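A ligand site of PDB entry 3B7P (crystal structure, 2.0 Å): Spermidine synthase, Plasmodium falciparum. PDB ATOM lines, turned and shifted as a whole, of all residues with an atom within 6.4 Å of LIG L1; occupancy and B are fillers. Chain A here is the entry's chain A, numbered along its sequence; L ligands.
OD2 of Asp 89 lies within salt-bridge range of N4 of LG2 L2 (2.8 Å).
The backbone NH (N) of Ala 166 is in hydrogen-bond range of a nitrogen (N2) of LIG L1 (3.0 Å).
OD2 of Asp 158 lies within salt-bridge range of N4 of LG2 L2, at 2.8 Å.
OE1 of Glu 109 sits at hydrogen-bond distance from O3 of LIG L1.
N of Gly 87 lies close to S1 of LIG L1, at 3.7 Å.
The backbone NH (N) of Ala 141 is in hydrogen-bond range of a nitrogen (N4) of LIG L1 (3.0 Å).
The backbone carbonyl oxygen (O) of Ser 159 sits at hydrogen-bond distance from a nitrogen (N3) of LG2 L2.
The side-chain carboxylate (OD1) of Asp 161 is in salt-bridge range of a nitrogen (N1) of LG2 L2 (2.9 Å).
N of Ser 160 is in hydrogen-bond range of O1 of LIG L1 (3.5 Å).
N5 of LIG L1 is in hydrogen-bond range of N of Ile 110.
A nitrogen (N3) of LIG L1 is in hydrogen-bond range of the side-chain carboxylate (OD1) of Asp 140 (2.8 Å).
A nitrogen (N3) of LIG L1 lies within hydrogen-bond range of the side-chain hydroxyl of Thr 168 (3.4 Å).
N3 of LIG L1 sits at hydrogen-bond distance from O of Pro 165 (3.3 Å).
The backbone NH (N) of Gly 88 lies close to a sulfur (S1) of LIG L1 (3.7 Å).
An oxygen (O2) of LIG L1 is in hydrogen-bond range of the side-chain amide nitrogen of Gln 34 (2.8 Å).
N4 of LG2 L2 lies close to S1 of LIG L1, 3.8 Å away.
The backbone carbonyl oxygen (O) of Val 85 lies within hydrogen-bond range of the backbone NH (N) of Asp 158.
The backbone NH of Gly 88 is in hydrogen-bond range of the side-chain carboxylate of Glu 109 (2.9 Å).
The backbone NH (N) of Gln 55 sits at hydrogen-bond distance from the backbone carbonyl oxygen (O) of Leu 48 (2.8 Å).
SG of Cys 108 sits at hydrogen-bond distance from O of Glu 139, at 3.2 Å.
OD1 of Asp 140 lies within hydrogen-bond range of N of Ser 142, 2.9 Å away.
OE2 of Glu 109 sits at hydrogen-bond distance from N of Asp 111, 2.7 Å away.
SG of Cys 108 lies close to N of Ala 141 (3.8 Å).
O of Glu 109 is in hydrogen-bond range of N of Glu 139, 3.2 Å away.
OD2 of Asp 89 lies close to S1 of LIG L1 (3.0 Å).
Merely in contact with LIG L1: Asp 158, Val 114, Gly 86, Leu 169, Cys 108, Gln 55, Asp 111, Glu 139, Leu 50 and Ser 159.
22 residues have an atom within 4 Å of LIG L1: Gln 34, Leu 50, Gln 55, Gly 86, Gly 87, Gly 88, Asp 89, Cys 108, Glu 109, Ile 110, Asp 111, Val 114, Glu 139, Asp 140, Ala 141, Asp 158, Ser 159, Ser 160, Pro 165, Ala 166, Thr 168 and Leu 169.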
ATOM      1  N   TYR A  33      14.727  -5.353  -6.768  1.00  0.00           N
ATOM      2  CA  TYR A  33      14.944  -3.901  -6.739  1.00  0.00           C
ATOM      3  C   TYR A  33      15.103  -3.294  -5.344  1.00  0.00           C
ATOM      4  O   TYR A  33      15.825  -2.322  -5.189  1.00  0.00           O
ATOM      5  CB  TYR A  33      13.817  -3.179  -7.490  1.00  0.00           C
ATOM      6  CG  TYR A  33      13.775  -3.530  -8.961  1.00  0.00           C
ATOM      7  CD1 TYR A  33      12.870  -4.473  -9.454  1.00  0.00           C
ATOM      8  CD2 TYR A  33      14.662  -2.946  -9.859  1.00  0.00           C
ATOM      9  CE1 TYR A  33      12.842  -4.814 -10.787  1.00  0.00           C
ATOM     10  CE2 TYR A  33      14.649  -3.293 -11.220  1.00  0.00           C
ATOM     11  CZ  TYR A  33      13.730  -4.228 -11.663  1.00  0.00           C
ATOM     12  OH  TYR A  33      13.692  -4.559 -12.992  1.00  0.00           O
ATOM     13  N   GLN A  34      14.427  -3.844  -4.339  1.00  0.00           N
ATOM     14  CA  GLN A  34      14.415  -3.180  -3.038  1.00  0.00           C
ATOM     15  C   GLN A  34      14.158  -4.128  -1.858  1.00  0.00           C
ATOM     16  O   GLN A  34      13.742  -5.259  -2.036  1.00  0.00           O
ATOM     17  CB  GLN A  34      13.425  -2.000  -3.056  1.00  0.00           C
ATOM     18  CG  GLN A  34      11.988  -2.346  -3.313  1.00  0.00           C
ATOM     19  CD  GLN A  34      11.228  -1.310  -4.160  1.00  0.00           C
ATOM     20  OE1 GLN A  34      11.556  -0.111  -4.192  1.00  0.00           O
ATOM     21  NE2 GLN A  34      10.189  -1.776  -4.847  1.00  0.00           N
ATOM     22  N   LEU A  48       3.620  -0.898   5.179  1.00  0.00           N
ATOM     23  CA  LEU A  48       4.502  -1.357   4.130  1.00  0.00           C
ATOM     24  C   LEU A  48       5.709  -0.443   4.061  1.00  0.00           C
ATOM     25  O   LEU A  48       5.580   0.776   4.026  1.00  0.00           O
ATOM     26  CB  LEU A  48       3.746  -1.404   2.784  1.00  0.00           C
ATOM     27  CG  LEU A  48       4.558  -1.659   1.498  1.00  0.00           C
ATOM     28  CD1 LEU A  48       5.119  -3.086   1.468  1.00  0.00           C
ATOM     29  CD2 LEU A  48       3.725  -1.379   0.257  1.00  0.00           C
ATOM     30  N   LEU A  50       9.634   0.130   2.129  1.00  0.00           N
ATOM     31  CA  LEU A  50      10.509  -0.190   1.009  1.00  0.00           C
ATOM     32  C   LEU A  50      11.795   0.598   1.177  1.00  0.00           C
ATOM     33  O   LEU A  50      11.765   1.822   1.263  1.00  0.00           O
ATOM     34  CB  LEU A  50       9.839   0.137  -0.331  1.00  0.00           C
ATOM     35  CG  LEU A  50       8.546  -0.597  -0.734  1.00  0.00           C
ATOM     36  CD1 LEU A  50       7.997  -0.074  -2.062  1.00  0.00           C
ATOM     37  CD2 LEU A  50       8.758  -2.107  -0.809  1.00  0.00           C
ATOM     38  N   GLN A  55       5.805   3.402   3.127  1.00  0.00           N
ATOM     39  CA  GLN A  55       5.057   3.639   1.887  1.00  0.00           C
ATOM     40  C   GLN A  55       3.597   3.861   2.213  1.00  0.00           C
ATOM     41  O   GLN A  55       2.934   4.714   1.636  1.00  0.00           O
ATOM     42  CB  GLN A  55       5.225   2.442   0.929  1.00  0.00           C
ATOM     43  CG  GLN A  55       6.669   2.123   0.611  1.00  0.00           C
ATOM     44  CD  GLN A  55       7.350   3.201  -0.222  1.00  0.00           C
ATOM     45  OE1 GLN A  55       8.446   3.679   0.117  1.00  0.00           O
ATOM     46  NE2 GLN A  55       6.723   3.568  -1.326  1.00  0.00           N
ATOM     47  N   LEU A  56       3.075   3.099   3.150  1.00  0.00           N
ATOM     48  CA  LEU A  56       1.724   3.329   3.587  1.00  0.00           C
ATOM     49  C   LEU A  56       1.487   2.676   4.929  1.00  0.00           C
ATOM     50  O   LEU A  56       2.272   1.832   5.356  1.00  0.00           O
ATOM     51  CB  LEU A  56       0.698   2.832   2.538  1.00  0.00           C
ATOM     52  CG  LEU A  56       0.654   1.344   2.153  1.00  0.00           C
ATOM     53  CD1 LEU A  56      -0.080   0.466   3.173  1.00  0.00           C
ATOM     54  CD2 LEU A  56      -0.029   1.210   0.814  1.00  0.00           C
ATOM     55  N   VAL A  85       1.704   5.150 -12.553  1.00  0.00           N
ATOM     56  CA  VAL A  85       3.123   4.812 -12.535  1.00  0.00           C
ATOM     57  C   VAL A  85       3.543   4.481 -11.109  1.00  0.00           C
ATOM     58  O   VAL A  85       3.213   5.221 -10.175  1.00  0.00           O
ATOM     59  CB  VAL A  85       4.010   5.953 -13.115  1.00  0.00           C
ATOM     60  CG1 VAL A  85       5.478   5.812 -12.658  1.00  0.00           C
ATOM     61  CG2 VAL A  85       3.934   5.962 -14.623  1.00  0.00           C
ATOM     62  N   GLY A  86       4.259   3.362 -10.940  1.00  0.00           N
ATOM     63  CA  GLY A  86       4.539   2.811  -9.613  1.00  0.00           C
ATOM     64  C   GLY A  86       3.249   2.287  -9.009  1.00  0.00           C
ATOM     65  O   GLY A  86       2.518   1.542  -9.660  1.00  0.00           O
ATOM     66  N   GLY A  87       2.977   2.688  -7.776  1.00  0.00           N
ATOM     67  CA  GLY A  87       1.696   2.377  -7.134  1.00  0.00           C
ATOM     68  C   GLY A  87       1.328   0.917  -6.929  1.00  0.00           C
ATOM     69  O   GLY A  87       0.135   0.590  -6.876  1.00  0.00           O
ATOM     70  N   GLY A  88       2.335   0.062  -6.752  1.00  0.00           N
ATOM     71  CA  GLY A  88       2.167  -1.391  -6.661  1.00  0.00           C
ATOM     72  C   GLY A  88       1.206  -1.885  -5.599  1.00  0.00           C
ATOM     73  O   GLY A  88       0.625  -2.955  -5.732  1.00  0.00           O
ATOM     74  N   ASP A  89       1.024  -1.104  -4.546  1.00  0.00           N
ATOM     75  CA  ASP A  89       0.083  -1.470  -3.460  1.00  0.00           C
ATOM     76  C   ASP A  89      -1.394  -1.488  -3.889  1.00  0.00           C
ATOM     77  O   ASP A  89      -2.223  -2.179  -3.279  1.00  0.00           O
ATOM     78  CB  ASP A  89       0.299  -0.525  -2.270  1.00  0.00           C
ATOM     79  CG  ASP A  89       0.300   0.929  -2.691  1.00  0.00           C
ATOM     80  OD1 ASP A  89      -0.790   1.473  -2.904  1.00  0.00           O
ATOM     81  OD2 ASP A  89       1.393   1.497  -2.857  1.00  0.00           O
ATOM     82  N   CYS A 108       1.993   0.601 -14.473  1.00  0.00           N
ATOM     83  CA  CYS A 108       3.365   0.199 -14.692  1.00  0.00           C
ATOM     84  C   CYS A 108       4.144   0.276 -13.365  1.00  0.00           C
ATOM     85  O   CYS A 108       4.451   1.369 -12.878  1.00  0.00           O
ATOM     86  CB  CYS A 108       4.001   1.086 -15.735  1.00  0.00           C
ATOM     87  SG  CYS A 108       5.656   0.613 -16.109  1.00  0.00           S
ATOM     88  N   GLU A 109       4.416  -0.897 -12.788  1.00  0.00           N
ATOM     89  CA  GLU A 109       5.108  -1.055 -11.501  1.00  0.00           C
ATOM     90  C   GLU A 109       6.352  -1.908 -11.760  1.00  0.00           C
ATOM     91  O   GLU A 109       6.231  -2.986 -12.311  1.00  0.00           O
ATOM     92  CB  GLU A 109       4.177  -1.731 -10.491  1.00  0.00           C
ATOM     93  CG  GLU A 109       4.882  -2.473  -9.342  1.00  0.00           C
ATOM     94  CD  GLU A 109       5.597  -1.559  -8.386  1.00  0.00           C
ATOM     95  OE1 GLU A 109       4.922  -0.780  -7.683  1.00  0.00           O
ATOM     96  OE2 GLU A 109       6.836  -1.619  -8.328  1.00  0.00           O
ATOM     97  N   ILE A 110       7.524  -1.401 -11.386  1.00  0.00           N
ATOM     98  CA  ILE A 110       8.789  -2.100 -11.633  1.00  0.00           C
ATOM     99  C   ILE A 110       8.946  -3.421 -10.835  1.00  0.00           C
ATOM    100  O   ILE A 110       9.590  -4.359 -11.297  1.00  0.00           O
ATOM    101  CB  ILE A 110      10.021  -1.159 -11.395  1.00  0.00           C
ATOM    102  CG1 ILE A 110      11.260  -1.660 -12.151  1.00  0.00           C
ATOM    103  CG2 ILE A 110      10.306  -0.936  -9.889  1.00  0.00           C
ATOM    104  CD1 ILE A 110      12.375  -0.645 -12.182  1.00  0.00           C
ATOM    105  N   ASP A 111       8.316  -3.485  -9.659  1.00  0.00           N
ATOM    106  CA  ASP A 111       8.583  -4.526  -8.675  1.00  0.00           C
ATOM    107  C   ASP A 111       7.336  -5.365  -8.400  1.00  0.00           C
ATOM    108  O   ASP A 111       6.490  -4.980  -7.570  1.00  0.00           O
ATOM    109  CB  ASP A 111       9.133  -3.904  -7.374  1.00  0.00           C
ATOM    110  CG  ASP A 111       9.826  -4.920  -6.476  1.00  0.00           C
ATOM    111  OD1 ASP A 111       9.570  -6.123  -6.627  1.00  0.00           O
ATOM    112  OD2 ASP A 111      10.633  -4.514  -5.591  1.00  0.00           O
ATOM    113  N   VAL A 114       6.118  -6.148  -4.816  1.00  0.00           N
ATOM    114  CA  VAL A 114       5.255  -5.166  -4.132  1.00  0.00           C
ATOM    115  C   VAL A 114       3.769  -5.489  -4.380  1.00  0.00           C
ATOM    116  O   VAL A 114       2.972  -5.539  -3.437  1.00  0.00           O
ATOM    117  CB  VAL A 114       5.595  -3.709  -4.529  1.00  0.00           C
ATOM    118  CG1 VAL A 114       4.574  -2.726  -3.940  1.00  0.00           C
ATOM    119  CG2 VAL A 114       6.992  -3.356  -4.045  1.00  0.00           C
ATOM    120  N   ILE A 115       3.419  -5.734  -5.641  1.00  0.00           N
ATOM    121  CA  ILE A 115       2.053  -6.085  -6.001  1.00  0.00           C
ATOM    122  C   ILE A 115       1.560  -7.332  -5.292  1.00  0.00           C
ATOM    123  O   ILE A 115       0.468  -7.327  -4.710  1.00  0.00           O
ATOM    124  CB  ILE A 115       1.881  -6.254  -7.532  1.00  0.00           C
ATOM    125  CG1 ILE A 115       2.211  -4.943  -8.254  1.00  0.00           C
ATOM    126  CG2 ILE A 115       0.460  -6.758  -7.857  1.00  0.00           C
ATOM    127  CD1 ILE A 115       2.057  -4.998  -9.755  1.00  0.00           C
ATOM    128  N   GLU A 139       7.543  -3.326 -15.249  1.00  0.00           N
ATOM    129  CA  GLU A 139       8.467  -2.602 -16.111  1.00  0.00           C
ATOM    130  C   GLU A 139       8.879  -1.309 -15.424  1.00  0.00           C
ATOM    131  O   GLU A 139       8.126  -0.762 -14.608  1.00  0.00           O
ATOM    132  CB  GLU A 139       7.749  -2.263 -17.414  1.00  0.00           C
ATOM    133  CG  GLU A 139       8.520  -2.489 -18.693  1.00  0.00           C
ATOM    134  CD  GLU A 139       7.602  -2.405 -19.910  1.00  0.00           C
ATOM    135  OE1 GLU A 139       6.510  -3.044 -19.893  1.00  0.00           O
ATOM    136  OE2 GLU A 139       7.957  -1.711 -20.890  1.00  0.00           O
ATOM    137  N   ASP A 140      10.080  -0.833 -15.743  1.00  0.00           N
ATOM    138  CA  ASP A 140      10.524   0.502 -15.378  1.00  0.00           C
ATOM    139  C   ASP A 140       9.680   1.502 -16.175  1.00  0.00           C
ATOM    140  O   ASP A 140       9.701   1.475 -17.404  1.00  0.00           O
ATOM    141  CB  ASP A 140      12.015   0.663 -15.719  1.00  0.00           C
ATOM    142  CG  ASP A 140      12.611   1.960 -15.172  1.00  0.00           C
ATOM    143  OD1 ASP A 140      11.894   2.972 -15.057  1.00  0.00           O
ATOM    144  OD2 ASP A 140      13.819   1.975 -14.859  1.00  0.00           O
ATOM    145  N   ALA A 141       8.927   2.360 -15.478  1.00  0.00           N
ATOM    146  CA  ALA A 141       8.047   3.334 -16.135  1.00  0.00           C
ATOM    147  C   ALA A 141       8.821   4.257 -17.072  1.00  0.00           C
ATOM    148  O   ALA A 141       8.269   4.771 -18.039  1.00  0.00           O
ATOM    149  CB  ALA A 141       7.279   4.118 -15.117  1.00  0.00           C
ATOM    150  N   SER A 142      10.112   4.439 -16.793  1.00  0.00           N
ATOM    151  CA  SER A 142      11.010   5.154 -17.693  1.00  0.00           C
ATOM    152  C   SER A 142      11.070   4.524 -19.101  1.00  0.00           C
ATOM    153  O   SER A 142      11.115   5.242 -20.108  1.00  0.00           O
ATOM    154  CB  SER A 142      12.405   5.274 -17.074  1.00  0.00           C
ATOM    155  OG  SER A 142      13.242   6.099 -17.862  1.00  0.00           O
ATOM    156  N   ASP A 158       2.661   7.533  -8.771  1.00  0.00           N
ATOM    157  CA  ASP A 158       2.676   7.121  -7.375  1.00  0.00           C
ATOM    158  C   ASP A 158       3.966   6.358  -7.074  1.00  0.00           C
ATOM    159  O   ASP A 158       3.961   5.154  -6.823  1.00  0.00           O
ATOM    160  CB  ASP A 158       1.444   6.263  -7.041  1.00  0.00           C
ATOM    161  CG  ASP A 158       1.393   5.827  -5.584  1.00  0.00           C
ATOM    162  OD1 ASP A 158       2.111   6.401  -4.750  1.00  0.00           O
ATOM    163  OD2 ASP A 158       0.627   4.897  -5.242  1.00  0.00           O
ATOM    164  N   SER A 159       5.080   7.089  -7.094  1.00  0.00           N
ATOM    165  CA  SER A 159       6.403   6.512  -6.943  1.00  0.00           C
ATOM    166  C   SER A 159       6.845   6.464  -5.498  1.00  0.00           C
ATOM    167  O   SER A 159       6.323   7.185  -4.638  1.00  0.00           O
ATOM    168  CB  SER A 159       7.411   7.351  -7.719  1.00  0.00           C
ATOM    169  OG  SER A 159       7.531   8.650  -7.149  1.00  0.00           O
ATOM    170  N   SER A 160       7.829   5.604  -5.234  1.00  0.00           N
ATOM    171  CA  SER A 160       8.652   5.714  -4.048  1.00  0.00           C
ATOM    172  C   SER A 160       9.606   6.912  -4.219  1.00  0.00           C
ATOM    173  O   SER A 160       9.536   7.650  -5.214  1.00  0.00           O
ATOM    174  CB  SER A 160       9.408   4.406  -3.809  1.00  0.00           C
ATOM    175  OG  SER A 160      10.015   3.929  -5.004  1.00  0.00           O
ATOM    176  N   ASP A 161      10.493   7.121  -3.247  1.00  0.00           N
ATOM    177  CA  ASP A 161      11.407   8.272  -3.257  1.00  0.00           C
ATOM    178  C   ASP A 161      12.590   8.122  -4.236  1.00  0.00           C
ATOM    179  O   ASP A 161      12.846   7.019  -4.704  1.00  0.00           O
ATOM    180  CB  ASP A 161      11.889   8.526  -1.832  1.00  0.00           C
ATOM    181  CG  ASP A 161      10.762   8.910  -0.915  1.00  0.00           C
ATOM    182  OD1 ASP A 161      10.056   9.898  -1.214  1.00  0.00           O
ATOM    183  OD2 ASP A 161      10.576   8.224   0.113  1.00  0.00           O
ATOM    184  N   GLY A 164      16.596   4.594  -4.915  1.00  0.00           N
ATOM    185  CA  GLY A 164      16.018   3.308  -5.288  1.00  0.00           C
ATOM    186  C   GLY A 164      15.624   3.302  -6.761  1.00  0.00           C
ATOM    187  O   GLY A 164      16.146   4.105  -7.544  1.00  0.00           O
ATOM    188  N   PRO A 165      14.716   2.394  -7.144  1.00  0.00           N
ATOM    189  CA  PRO A 165      14.267   2.312  -8.551  1.00  0.00           C
ATOM    190  C   PRO A 165      13.578   3.570  -9.103  1.00  0.00           C
ATOM    191  O   PRO A 165      13.550   3.769 -10.306  1.00  0.00           O
ATOM    192  CB  PRO A 165      13.302   1.110  -8.554  1.00  0.00           C
ATOM    193  CG  PRO A 165      12.871   0.959  -7.112  1.00  0.00           C
ATOM    194  CD  PRO A 165      14.066   1.373  -6.306  1.00  0.00           C
ATOM    195  N   ALA A 166      13.004   4.406  -8.222  1.00  0.00           N
ATOM    196  CA  ALA A 166      12.332   5.640  -8.641  1.00  0.00           C
ATOM    197  C   ALA A 166      13.315   6.745  -9.024  1.00  0.00           C
ATOM    198  O   ALA A 166      12.901   7.864  -9.330  1.00  0.00           O
ATOM    199  CB  ALA A 166      11.369   6.114  -7.567  1.00  0.00           C
ATOM    200  N   GLU A 167      14.590   6.408  -9.016  1.00  0.00           N
ATOM    201  CA  GLU A 167      15.698   7.261  -9.456  1.00  0.00           C
ATOM    202  C   GLU A 167      15.443   7.876 -10.842  1.00  0.00           C
ATOM    203  O   GLU A 167      15.726   9.062 -11.055  1.00  0.00           O
ATOM    204  CB  GLU A 167      16.974   6.432  -9.462  1.00  0.00           C
ATOM    205  CG  GLU A 167      18.216   7.094 -10.044  1.00  0.00           C
ATOM    206  CD  GLU A 167      19.493   6.519  -9.481  1.00  0.00           C
ATOM    207  OE1 GLU A 167      20.347   7.308  -9.022  1.00  0.00           O
ATOM    208  OE2 GLU A 167      19.642   5.273  -9.485  1.00  0.00           O
ATOM    209  N   THR A 168      14.896   7.058 -11.746  1.00  0.00           N
ATOM    210  CA  THR A 168      14.621   7.433 -13.147  1.00  0.00           C
ATOM    211  C   THR A 168      13.336   8.263 -13.353  1.00  0.00           C
ATOM    212  O   THR A 168      13.056   8.689 -14.481  1.00  0.00           O
ATOM    213  CB  THR A 168      14.531   6.177 -14.054  1.00  0.00           C
ATOM    214  OG1 THR A 168      13.487   5.309 -13.574  1.00  0.00           O
ATOM    215  CG2 THR A 168      15.847   5.407 -14.064  1.00  0.00           C
ATOM    216  N   LEU A 169      12.564   8.498 -12.287  1.00  0.00           N
ATOM    217  CA  LEU A 169      11.274   9.191 -12.404  1.00  0.00           C
ATOM    218  C   LEU A 169      11.336  10.659 -11.945  1.00  0.00           C
ATOM    219  O   LEU A 169      10.305  11.339 -11.848  1.00  0.00           O
ATOM    220  CB  LEU A 169      10.188   8.434 -11.611  1.00  0.00           C
ATOM    221  CG  LEU A 169      10.107   6.894 -11.763  1.00  0.00           C
ATOM    222  CD1 LEU A 169       9.019   6.324 -10.888  1.00  0.00           C
ATOM    223  CD2 LEU A 169       9.929   6.441 -13.215  1.00  0.00           C
HETATM  224  C1  LIG L   1       4.526   1.348  -2.951  1.00  0.00           C
HETATM  225  S1  LIG L   1       3.911   2.343  -4.264  1.00  0.00           S
HETATM  226  C2  LIG L   1       5.373   3.030  -4.987  1.00  0.00           C
HETATM  227  C3  LIG L   1       5.935   2.078  -6.034  1.00  0.00           C
HETATM  228  O1  LIG L   1       6.796   2.752  -6.973  1.00  0.00           O
HETATM  229  C4  LIG L   1       8.048   0.960  -6.354  1.00  0.00           C
HETATM  230  O2  LIG L   1       8.473  -0.385  -6.639  1.00  0.00           O
HETATM  231  C5  LIG L   1       6.840   1.011  -5.438  1.00  0.00           C
HETATM  232  O3  LIG L   1       6.185  -0.249  -5.432  1.00  0.00           O
HETATM  233  C6  LIG L   1       7.522   1.710  -7.566  1.00  0.00           C
HETATM  234  N1  LIG L   1       8.591   2.222  -8.465  1.00  0.00           N
HETATM  235  C7  LIG L   1       9.758   2.773  -8.115  1.00  0.00           C
HETATM  236  N2  LIG L   1      10.496   3.099  -9.222  1.00  0.00           N
HETATM  237  C8  LIG L   1       9.755   2.750 -10.312  1.00  0.00           C
HETATM  238  C9  LIG L   1       9.900   2.798 -11.781  1.00  0.00           C
HETATM  239  N3  LIG L   1      11.023   3.322 -12.368  1.00  0.00           N
HETATM  240  N4  LIG L   1       8.877   2.307 -12.520  1.00  0.00           N
HETATM  241  C10 LIG L   1       7.759   1.772 -11.972  1.00  0.00           C
HETATM  242  N5  LIG L   1       7.565   1.692 -10.641  1.00  0.00           N
HETATM  243  C11 LIG L   1       8.501   2.161  -9.792  1.00  0.00           C
HETATM  244  N1  LG2 L   2       9.645  12.736  -0.867  1.00  0.00           N
HETATM  245  C1  LG2 L   2       9.986  12.733   0.582  1.00  0.00           C
HETATM  246  C2  LG2 L   2       8.929  12.004   1.452  1.00  0.00           C
HETATM  247  C3  LG2 L   2       9.393  10.563   1.780  1.00  0.00           C
HETATM  248  N2  LG2 L   2       8.333   9.533   1.882  1.00  0.00           N
HETATM  249  C4  LG2 L   2       7.510   9.447   0.662  1.00  0.00           C
HETATM  250  C5  LG2 L   2       7.005   8.021   0.414  1.00  0.00           C
HETATM  251  C6  LG2 L   2       6.206   7.997  -0.887  1.00  0.00           C
HETATM  252  C7  LG2 L   2       5.705   6.594  -1.237  1.00  0.00           C
HETATM  253  N3  LG2 L   2       4.512   6.701  -2.101  1.00  0.00           N
HETATM  254  C8  LG2 L   2       4.052   5.392  -2.577  1.00  0.00           C
HETATM  255  C9  LG2 L   2       3.320   4.611  -1.487  1.00  0.00           C
HETATM  256  C10 LG2 L   2       1.811   4.876  -1.452  1.00  0.00           C
HETATM  257  N4  LG2 L   2       1.130   4.242  -2.592  1.00  0.00           N
